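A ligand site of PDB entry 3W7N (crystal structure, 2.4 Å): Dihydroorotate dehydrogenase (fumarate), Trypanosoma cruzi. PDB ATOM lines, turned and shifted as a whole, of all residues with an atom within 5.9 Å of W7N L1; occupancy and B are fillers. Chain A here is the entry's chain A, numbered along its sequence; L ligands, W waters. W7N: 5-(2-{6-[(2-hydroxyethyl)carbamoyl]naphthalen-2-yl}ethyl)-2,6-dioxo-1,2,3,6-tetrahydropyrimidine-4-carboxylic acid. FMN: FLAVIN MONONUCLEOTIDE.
Water W1 bridges an oxygen (OAF) of W7N L1 and the side-chain amide oxygen of Asn 68.
NH2 of Arg 51 touches CAH of W7N L1 (3.9 Å). Ser 69 touches W7N L1. Ser 130 touches W7N L1. Pro 132 touches W7N L1. CG of Lys 215 touches CAN of W7N L1, 3.7 Å away. Hydrophobic or aromatic side chains within 4 Å of W7N L1: Met 70, Leu 72 and Pro 132. Within 4 Å of W7N L1: Lys 44, Arg 51, Asn 54, Asn 68, Ser 69, Met 70, Gly 71, Leu 72, Asn 128, Ser 130, Pro 132, Asn 195, Ser 196 and Lys 215.
The backbone NH (N) of Met 70 sits at hydrogen-bond distance from the side-chain amide oxygen (OD1) of Asn 68, at 3.5 Å. The side-chain amide oxygen (OD1) of Asn 195 sits at hydrogen-bond distance from the side-chain hydroxyl (OG) of Ser 196, 3.1 Å away. ND2 of Asn 195 sits at hydrogen-bond distance from OG of Ser 130 (2.9 Å). The side-chain amide nitrogen of Asn 54 lies close to the backbone NH of Gly 71. The backbone carbonyl oxygen of Met 70 sits at hydrogen-bond distance from the backbone NH of Asn 54 (3.0 Å). The backbone carbonyl oxygen (O) of Asn 128 is in hydrogen-bond range of the side-chain sulfur (SG) of Cys 131. ND2 of Asn 128 sits at hydrogen-bond distance from OG of Ser 45. ND2 of Asn 54 lies within hydrogen-bond range of O of Ser 69 (2.7 Å).
A nitrogen (N3) of FMN L2 sits close to an oxygen (OAD) of W7N L1, 3.4 Å away.
A nitrogen (NAR) of W7N L1 is in hydrogen-bond range of the side-chain amide oxygen of Asn 68 (2.7 Å). OG of Ser 196 is in hydrogen-bond range of OAC of W7N L1, 2.7 Å away. OD1 of Asn 195 lies within hydrogen-bond range of NAS of W7N L1 (2.9 Å). N of Gly 71 lies within hydrogen-bond range of OAF of W7N L1 (2.9 Å). The backbone NH (N) of Leu 72 sits at hydrogen-bond distance from an oxygen (OAA) of W7N L1. An oxygen (OAA) of W7N L1 is in salt-bridge range of the side-chain amino group (NZ) of Lys 44 (3.0 Å). The backbone NH (N) of Met 70 sits at hydrogen-bond distance from an oxygen (OAF) of W7N L1, at 3.0 Å. An oxygen (OAD) of W7N L1 lies within hydrogen-bond range of the side-chain amide nitrogen (ND2) of Asn 128 (3.2 Å). A nitrogen (NAQ) of W7N L1 sits close to the side-chain amide nitrogen of Asn 54, at 3.3 Å. The side-chain amide nitrogen of Asn 195 sits at hydrogen-bond distance from an oxygen (O2) of FMN L2, at 3.0 Å. O4 of FMN L2 is in hydrogen-bond range of NZ of Lys 44 (2.8 Å). An oxygen (O2) of FMN L2 is in hydrogen-bond range of the side-chain amide nitrogen (ND2) of Asn 128 (2.9 Å). The side-chain hydroxyl (OG) of Ser 45 is in hydrogen-bond range of a nitrogen (N3) of FMN L2 (3.2 Å). O2 of FMN L2 is in hydrogen-bond range of NZ of Lys 165.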
ATOM      1  N   LYS A  44      10.061  -6.532  -9.864  1.00  0.00           N
ATOM      2  CA  LYS A  44      10.366  -6.962 -11.224  1.00  0.00           C
ATOM      3  C   LYS A  44      11.776  -7.509 -11.207  1.00  0.00           C
ATOM      4  O   LYS A  44      12.615  -6.984 -10.505  1.00  0.00           O
ATOM      5  CB  LYS A  44      10.262  -5.763 -12.169  1.00  0.00           C
ATOM      6  CG  LYS A  44      10.770  -5.934 -13.616  1.00  0.00           C
ATOM      7  CD  LYS A  44      10.335  -7.222 -14.318  1.00  0.00           C
ATOM      8  CE  LYS A  44      11.109  -7.464 -15.624  1.00  0.00           C
ATOM      9  NZ  LYS A  44      10.330  -8.314 -16.588  1.00  0.00           N
ATOM     10  N   SER A  45      12.018  -8.576 -11.973  1.00  0.00           N
ATOM     11  CA  SER A  45      13.355  -9.166 -12.115  1.00  0.00           C
ATOM     12  C   SER A  45      14.304  -8.108 -12.717  1.00  0.00           C
ATOM     13  O   SER A  45      14.061  -7.577 -13.782  1.00  0.00           O
ATOM     14  CB  SER A  45      13.350 -10.419 -12.987  1.00  0.00           C
ATOM     15  OG  SER A  45      12.874 -11.557 -12.314  1.00  0.00           O
ATOM     16  N   ARG A  51      17.310  -1.428 -18.135  1.00  0.00           N
ATOM     17  CA  ARG A  51      17.019  -1.900 -19.480  1.00  0.00           C
ATOM     18  C   ARG A  51      15.678  -1.352 -19.984  1.00  0.00           C
ATOM     19  O   ARG A  51      14.736  -1.212 -19.215  1.00  0.00           O
ATOM     20  CB  ARG A  51      16.965  -3.430 -19.562  1.00  0.00           C
ATOM     21  CG  ARG A  51      18.258  -4.131 -19.240  1.00  0.00           C
ATOM     22  CD  ARG A  51      18.028  -5.615 -19.037  1.00  0.00           C
ATOM     23  NE  ARG A  51      17.342  -6.241 -20.163  1.00  0.00           N
ATOM     24  CZ  ARG A  51      17.967  -6.657 -21.260  1.00  0.00           C
ATOM     25  NH1 ARG A  51      19.281  -6.519 -21.360  1.00  0.00           N
ATOM     26  NH2 ARG A  51      17.283  -7.198 -22.239  1.00  0.00           N
ATOM     27  N   ASN A  54      12.508  -5.143 -24.927  1.00  0.00           N
ATOM     28  CA  ASN A  54      12.138  -5.350 -26.314  1.00  0.00           C
ATOM     29  C   ASN A  54      11.177  -4.256 -26.791  1.00  0.00           C
ATOM     30  O   ASN A  54      10.540  -3.571 -25.967  1.00  0.00           O
ATOM     31  CB  ASN A  54      11.462  -6.715 -26.458  1.00  0.00           C
ATOM     32  CG  ASN A  54      12.425  -7.861 -26.319  1.00  0.00           C
ATOM     33  OD1 ASN A  54      13.644  -7.658 -26.463  1.00  0.00           O
ATOM     34  ND2 ASN A  54      11.918  -9.052 -26.041  1.00  0.00           N
ATOM     35  N   ASN A  68       4.020 -13.115 -23.731  1.00  0.00           N
ATOM     36  CA  ASN A  68       4.883 -11.951 -23.528  1.00  0.00           C
ATOM     37  C   ASN A  68       6.284 -12.201 -23.993  1.00  0.00           C
ATOM     38  O   ASN A  68       6.856 -13.295 -23.775  1.00  0.00           O
ATOM     39  CB  ASN A  68       4.899 -11.461 -22.036  1.00  0.00           C
ATOM     40  CG  ASN A  68       5.931 -12.202 -21.161  1.00  0.00           C
ATOM     41  OD1 ASN A  68       7.166 -11.962 -21.211  1.00  0.00           O
ATOM     42  ND2 ASN A  68       5.426 -13.099 -20.366  1.00  0.00           N
ATOM     43  N   SER A  69       6.874 -11.171 -24.587  1.00  0.00           N
ATOM     44  CA  SER A  69       8.349 -11.182 -24.675  1.00  0.00           C
ATOM     45  C   SER A  69       8.950  -9.811 -24.321  1.00  0.00           C
ATOM     46  O   SER A  69       9.390  -9.037 -25.189  1.00  0.00           O
ATOM     47  CB  SER A  69       8.882 -11.723 -25.995  1.00  0.00           C
ATOM     48  OG  SER A  69      10.266 -11.387 -26.066  1.00  0.00           O
ATOM     49  N   MET A  70       8.900  -9.524 -23.020  1.00  0.00           N
ATOM     50  CA  MET A  70       9.249  -8.193 -22.502  1.00  0.00           C
ATOM     51  C   MET A  70      10.762  -7.869 -22.676  1.00  0.00           C
ATOM     52  O   MET A  70      11.151  -6.703 -22.754  1.00  0.00           O
ATOM     53  CB  MET A  70       8.897  -8.123 -21.031  1.00  0.00           C
ATOM     54  CG  MET A  70       7.479  -8.495 -20.684  1.00  0.00           C
ATOM     55  SD  MET A  70       6.280  -7.418 -21.462  1.00  0.00           S
ATOM     56  CE  MET A  70       6.246  -5.990 -20.393  1.00  0.00           C
ATOM     57  N   GLY A  71      11.614  -8.893 -22.743  1.00  0.00           N
ATOM     58  CA  GLY A  71      13.056  -8.707 -22.670  1.00  0.00           C
ATOM     59  C   GLY A  71      13.620  -8.016 -21.431  1.00  0.00           C
ATOM     60  O   GLY A  71      14.571  -7.272 -21.537  1.00  0.00           O
ATOM     61  N   LEU A  72      12.995  -8.220 -20.262  1.00  0.00           N
ATOM     62  CA  LEU A  72      13.574  -7.764 -18.992  1.00  0.00           C
ATOM     63  C   LEU A  72      13.787  -6.237 -18.874  1.00  0.00           C
ATOM     64  O   LEU A  72      14.856  -5.780 -18.478  1.00  0.00           O
ATOM     65  CB  LEU A  72      14.920  -8.451 -18.820  1.00  0.00           C
ATOM     66  CG  LEU A  72      15.257  -9.039 -17.478  1.00  0.00           C
ATOM     67  CD1 LEU A  72      14.017  -9.542 -16.756  1.00  0.00           C
ATOM     68  CD2 LEU A  72      16.245 -10.171 -17.732  1.00  0.00           C
ATOM     69  N   PRO A  73      12.761  -5.464 -19.245  1.00  0.00           N
ATOM     70  CA  PRO A  73      12.819  -4.035 -18.921  1.00  0.00           C
ATOM     71  C   PRO A  73      12.671  -3.900 -17.430  1.00  0.00           C
ATOM     72  O   PRO A  73      11.835  -4.569 -16.849  1.00  0.00           O
ATOM     73  CB  PRO A  73      11.564  -3.471 -19.568  1.00  0.00           C
ATOM     74  CG  PRO A  73      10.594  -4.632 -19.527  1.00  0.00           C
ATOM     75  CD  PRO A  73      11.421  -5.903 -19.679  1.00  0.00           C
ATOM     76  N   SER A 100      17.532 -11.218 -11.944  1.00  0.00           N
ATOM     77  CA  SER A 100      17.669 -12.064 -13.098  1.00  0.00           C
ATOM     78  C   SER A 100      18.797 -11.623 -13.982  1.00  0.00           C
ATOM     79  O   SER A 100      18.595 -11.393 -15.179  1.00  0.00           O
ATOM     80  CB  SER A 100      16.351 -12.130 -13.869  1.00  0.00           C
ATOM     81  OG  SER A 100      16.559 -12.822 -15.099  1.00  0.00           O
ATOM     82  N   LEU A 102      22.147 -11.511 -16.304  1.00  0.00           N
ATOM     83  CA  LEU A 102      22.319 -12.148 -17.634  1.00  0.00           C
ATOM     84  C   LEU A 102      23.529 -13.081 -17.721  1.00  0.00           C
ATOM     85  O   LEU A 102      23.783 -13.691 -18.746  1.00  0.00           O
ATOM     86  CB  LEU A 102      22.416 -11.085 -18.747  1.00  0.00           C
ATOM     87  CG  LEU A 102      21.246 -10.098 -19.000  1.00  0.00           C
ATOM     88  CD1 LEU A 102      21.348  -9.487 -20.399  1.00  0.00           C
ATOM     89  CD2 LEU A 102      19.876 -10.743 -18.792  1.00  0.00           C
ATOM     90  N   ASN A 128      15.891 -15.756 -10.380  1.00  0.00           N
ATOM     91  CA  ASN A 128      15.222 -16.237 -11.555  1.00  0.00           C
ATOM     92  C   ASN A 128      16.119 -17.107 -12.482  1.00  0.00           C
ATOM     93  O   ASN A 128      17.057 -16.599 -13.104  1.00  0.00           O
ATOM     94  CB  ASN A 128      14.615 -15.040 -12.300  1.00  0.00           C
ATOM     95  CG  ASN A 128      13.784 -15.438 -13.495  1.00  0.00           C
ATOM     96  OD1 ASN A 128      13.777 -16.587 -13.886  1.00  0.00           O
ATOM     97  ND2 ASN A 128      13.092 -14.472 -14.096  1.00  0.00           N
ATOM     98  N   SER A 130      14.856 -19.192 -14.929  1.00  0.00           N
ATOM     99  CA  SER A 130      14.160 -19.404 -16.202  1.00  0.00           C
ATOM    100  C   SER A 130      14.498 -18.191 -17.040  1.00  0.00           C
ATOM    101  O   SER A 130      13.610 -17.495 -17.553  1.00  0.00           O
ATOM    102  CB  SER A 130      12.633 -19.586 -15.992  1.00  0.00           C
ATOM    103  OG  SER A 130      12.142 -19.261 -14.657  1.00  0.00           O
ATOM    104  N   CYS A 131      15.806 -17.918 -17.123  1.00  0.00           N
ATOM    105  CA  CYS A 131      16.374 -16.784 -17.866  1.00  0.00           C
ATOM    106  C   CYS A 131      17.436 -17.263 -18.871  1.00  0.00           C
ATOM    107  O   CYS A 131      18.013 -18.340 -18.666  1.00  0.00           O
ATOM    108  CB  CYS A 131      16.944 -15.712 -16.903  1.00  0.00           C
ATOM    109  SG  CYS A 131      18.471 -16.095 -15.988  1.00  0.00           S
ATOM    110  N   PRO A 132      17.694 -16.473 -19.949  1.00  0.00           N
ATOM    111  CA  PRO A 132      18.732 -16.871 -20.915  1.00  0.00           C
ATOM    112  C   PRO A 132      20.186 -16.822 -20.359  1.00  0.00           C
ATOM    113  O   PRO A 132      20.485 -16.007 -19.465  1.00  0.00           O
ATOM    114  CB  PRO A 132      18.545 -15.863 -22.073  1.00  0.00           C
ATOM    115  CG  PRO A 132      17.905 -14.678 -21.433  1.00  0.00           C
ATOM    116  CD  PRO A 132      17.005 -15.242 -20.365  1.00  0.00           C
ATOM    117  N   LYS A 165      13.139 -19.455  -8.916  1.00  0.00           N
ATOM    118  CA  LYS A 165      11.996 -19.490  -9.862  1.00  0.00           C
ATOM    119  C   LYS A 165      12.319 -20.440 -11.015  1.00  0.00           C
ATOM    120  O   LYS A 165      13.290 -20.196 -11.756  1.00  0.00           O
ATOM    121  CB  LYS A 165      11.678 -18.038 -10.323  1.00  0.00           C
ATOM    122  CG  LYS A 165      10.570 -17.809 -11.342  1.00  0.00           C
ATOM    123  CD  LYS A 165       9.179 -17.997 -10.796  1.00  0.00           C
ATOM    124  CE  LYS A 165       8.086 -17.546 -11.765  1.00  0.00           C
ATOM    125  NZ  LYS A 165       8.115 -16.104 -12.176  1.00  0.00           N
ATOM    126  N   ASN A 195       7.449 -20.610 -14.174  1.00  0.00           N
ATOM    127  CA  ASN A 195       7.553 -19.434 -15.003  1.00  0.00           C
ATOM    128  C   ASN A 195       6.673 -19.691 -16.219  1.00  0.00           C
ATOM    129  O   ASN A 195       6.026 -20.763 -16.307  1.00  0.00           O
ATOM    130  CB  ASN A 195       9.013 -19.207 -15.460  1.00  0.00           C
ATOM    131  CG  ASN A 195       9.318 -17.744 -15.738  1.00  0.00           C
ATOM    132  OD1 ASN A 195       8.765 -17.143 -16.663  1.00  0.00           O
ATOM    133  ND2 ASN A 195      10.145 -17.143 -14.906  1.00  0.00           N
ATOM    134  N   SER A 196       6.624 -18.735 -17.156  1.00  0.00           N
ATOM    135  CA  SER A 196       5.812 -18.922 -18.341  1.00  0.00           C
ATOM    136  C   SER A 196       6.176 -20.186 -19.134  1.00  0.00           C
ATOM    137  O   SER A 196       7.337 -20.586 -19.223  1.00  0.00           O
ATOM    138  CB  SER A 196       5.825 -17.667 -19.196  1.00  0.00           C
ATOM    139  OG  SER A 196       7.122 -17.125 -19.246  1.00  0.00           O
ATOM    140  N   PRO A 214       8.493  -8.686 -30.795  1.00  0.00           N
ATOM    141  CA  PRO A 214       9.790  -9.382 -30.740  1.00  0.00           C
ATOM    142  C   PRO A 214       9.718 -10.873 -31.123  1.00  0.00           C
ATOM    143  O   PRO A 214       8.649 -11.500 -31.007  1.00  0.00           O
ATOM    144  CB  PRO A 214      10.191  -9.280 -29.245  1.00  0.00           C
ATOM    145  CG  PRO A 214       9.316  -8.217 -28.683  1.00  0.00           C
ATOM    146  CD  PRO A 214       8.050  -8.257 -29.453  1.00  0.00           C
ATOM    147  N   LYS A 215      10.871 -11.420 -31.551  1.00  0.00           N
ATOM    148  CA  LYS A 215      11.061 -12.878 -31.720  1.00  0.00           C
ATOM    149  C   LYS A 215      10.080 -13.514 -32.704  1.00  0.00           C
ATOM    150  O   LYS A 215       9.651 -14.653 -32.515  1.00  0.00           O
ATOM    151  CB  LYS A 215      10.927 -13.576 -30.374  1.00  0.00           C
ATOM    152  CG  LYS A 215      12.053 -13.289 -29.380  1.00  0.00           C
ATOM    153  CD  LYS A 215      11.894 -14.174 -28.140  1.00  0.00           C
ATOM    154  CE  LYS A 215      12.089 -15.660 -28.529  1.00  0.00           C
ATOM    155  NZ  LYS A 215      11.728 -16.650 -27.495  1.00  0.00           N
ATOM    156  N   GLY A 220       6.427 -16.148 -23.986  1.00  0.00           N
ATOM    157  CA  GLY A 220       6.082 -17.067 -22.895  1.00  0.00           C
ATOM    158  C   GLY A 220       4.598 -16.968 -22.710  1.00  0.00           C
ATOM    159  O   GLY A 220       4.030 -15.870 -22.858  1.00  0.00           O
HETATM  160  OAA W7N L   1      10.868  -9.896 -19.076  1.00  0.00           O
HETATM  161  CAT W7N L   1      10.574 -10.965 -19.699  1.00  0.00           C
HETATM  162  OAF W7N L   1      10.571 -10.979 -20.962  1.00  0.00           O
HETATM  163  CAY W7N L   1      10.196 -12.157 -19.025  1.00  0.00           C
HETATM  164  NAR W7N L   1       8.952 -12.753 -19.388  1.00  0.00           N
HETATM  165  CAZ W7N L   1       8.509 -13.941 -18.800  1.00  0.00           C
HETATM  166  OAC W7N L   1       7.439 -14.466 -19.112  1.00  0.00           O
HETATM  167  NAS W7N L   1       9.274 -14.539 -17.875  1.00  0.00           N
HETATM  168  CBA W7N L   1      10.526 -14.016 -17.489  1.00  0.00           C
HETATM  169  OAD W7N L   1      11.165 -14.609 -16.593  1.00  0.00           O
HETATM  170  CAX W7N L   1      10.977 -12.805 -18.061  1.00  0.00           C
HETATM  171  CAP W7N L   1      12.239 -12.284 -17.665  1.00  0.00           C
HETATM  172  CAO W7N L   1      13.405 -13.246 -18.151  1.00  0.00           C
HETATM  173  CAV W7N L   1      13.614 -13.003 -19.492  1.00  0.00           C
HETATM  174  CAK W7N L   1      14.708 -12.222 -19.853  1.00  0.00           C
HETATM  175  CAG W7N L   1      12.735 -13.498 -20.461  1.00  0.00           C
HETATM  176  CAI W7N L   1      12.923 -13.227 -21.805  1.00  0.00           C
HETATM  177  CBC W7N L   1      14.023 -12.458 -22.164  1.00  0.00           C
HETATM  178  CAL W7N L   1      14.208 -12.195 -23.497  1.00  0.00           C
HETATM  179  CBB W7N L   1      14.931 -11.941 -21.192  1.00  0.00           C
HETATM  180  CAJ W7N L   1      16.034 -11.163 -21.553  1.00  0.00           C
HETATM  181  CAH W7N L   1      16.201 -10.889 -22.917  1.00  0.00           C
HETATM  182  CAW W7N L   1      15.303 -11.408 -23.879  1.00  0.00           C
HETATM  183  CAU W7N L   1      15.456 -11.142 -25.250  1.00  0.00           C
HETATM  184  OAB W7N L   1      16.526 -10.700 -25.669  1.00  0.00           O
HETATM  185  NAQ W7N L   1      14.338 -11.338 -26.006  1.00  0.00           N
HETATM  186  CAN W7N L   1      14.295 -11.110 -27.463  1.00  0.00           C
HETATM  187  CAM W7N L   1      15.679 -11.327 -28.148  1.00  0.00           C
HETATM  188  OAE W7N L   1      16.040 -12.728 -28.231  1.00  0.00           O
HETATM  189  N1  FMN L   2       8.642 -14.183 -14.377  1.00  0.00           N
HETATM  190  C2  FMN L   2       9.817 -13.836 -13.828  1.00  0.00           C
HETATM  191  O2  FMN L   2      10.400 -14.695 -13.154  1.00  0.00           O
HETATM  192  N3  FMN L   2      10.397 -12.630 -13.973  1.00  0.00           N
HETATM  193  C4  FMN L   2       9.799 -11.660 -14.656  1.00  0.00           C
HETATM  194  O4  FMN L   2      10.284 -10.517 -14.790  1.00  0.00           O
HETATM  195  C4A FMN L   2       8.517 -11.977 -15.282  1.00  0.00           C
HETATM  196  N5  FMN L   2       7.907 -11.040 -15.988  1.00  0.00           N
HETATM  197  C5A FMN L   2       6.732 -11.262 -16.560  1.00  0.00           C
HETATM  198  C6  FMN L   2       6.138 -10.219 -17.246  1.00  0.00           C
HETATM  199  C7  FMN L   2       4.878 -10.447 -17.778  1.00  0.00           C
HETATM  200  C7M FMN L   2       4.277  -9.298 -18.534  1.00  0.00           C
HETATM  201  C8  FMN L   2       4.212 -11.779 -17.653  1.00  0.00           C
HETATM  202  C8M FMN L   2       2.860 -12.113 -18.269  1.00  0.00           C
HETATM  203  C9  FMN L   2       4.834 -12.801 -16.973  1.00  0.00           C
HETATM  204  C9A FMN L   2       6.061 -12.578 -16.417  1.00  0.00           C
HETATM  205  N10 FMN L   2       6.701 -13.614 -15.675  1.00  0.00           N
HETATM  206  C10 FMN L   2       7.945 -13.316 -15.093  1.00  0.00           C
HETATM  207  C1' FMN L   2       6.047 -14.909 -15.558  1.00  0.00           C
HETATM  208  C2' FMN L   2       5.109 -14.824 -14.391  1.00  0.00           C
HETATM  209  O2' FMN L   2       5.928 -14.458 -13.260  1.00  0.00           O
HETATM  210  C3' FMN L   2       4.519 -16.186 -14.186  1.00  0.00           C
HETATM  211  O3' FMN L   2       5.638 -16.991 -13.869  1.00  0.00           O
HETATM  212  C4' FMN L   2       3.799 -16.681 -15.456  1.00  0.00           C
HETATM  213  O4' FMN L   2       3.187 -15.567 -16.144  1.00  0.00           O
HETATM  214  C5' FMN L   2       2.706 -17.705 -15.122  1.00  0.00           C
HETATM  215  O5' FMN L   2       1.741 -17.115 -14.250  1.00  0.00           O
HETATM  216  P   FMN L   2       0.218 -16.766 -14.669  1.00  0.00           P
HETATM  217  O1P FMN L   2      -0.518 -16.409 -13.418  1.00  0.00           O
HETATM  218  O2P FMN L   2      -0.229 -18.073 -15.233  1.00  0.00           O
HETATM  219  O3P FMN L   2       0.300 -15.671 -15.654  1.00  0.00           O
HETATM  220  O   HOH W   1       9.577 -13.213 -22.335  1.00  0.00           O
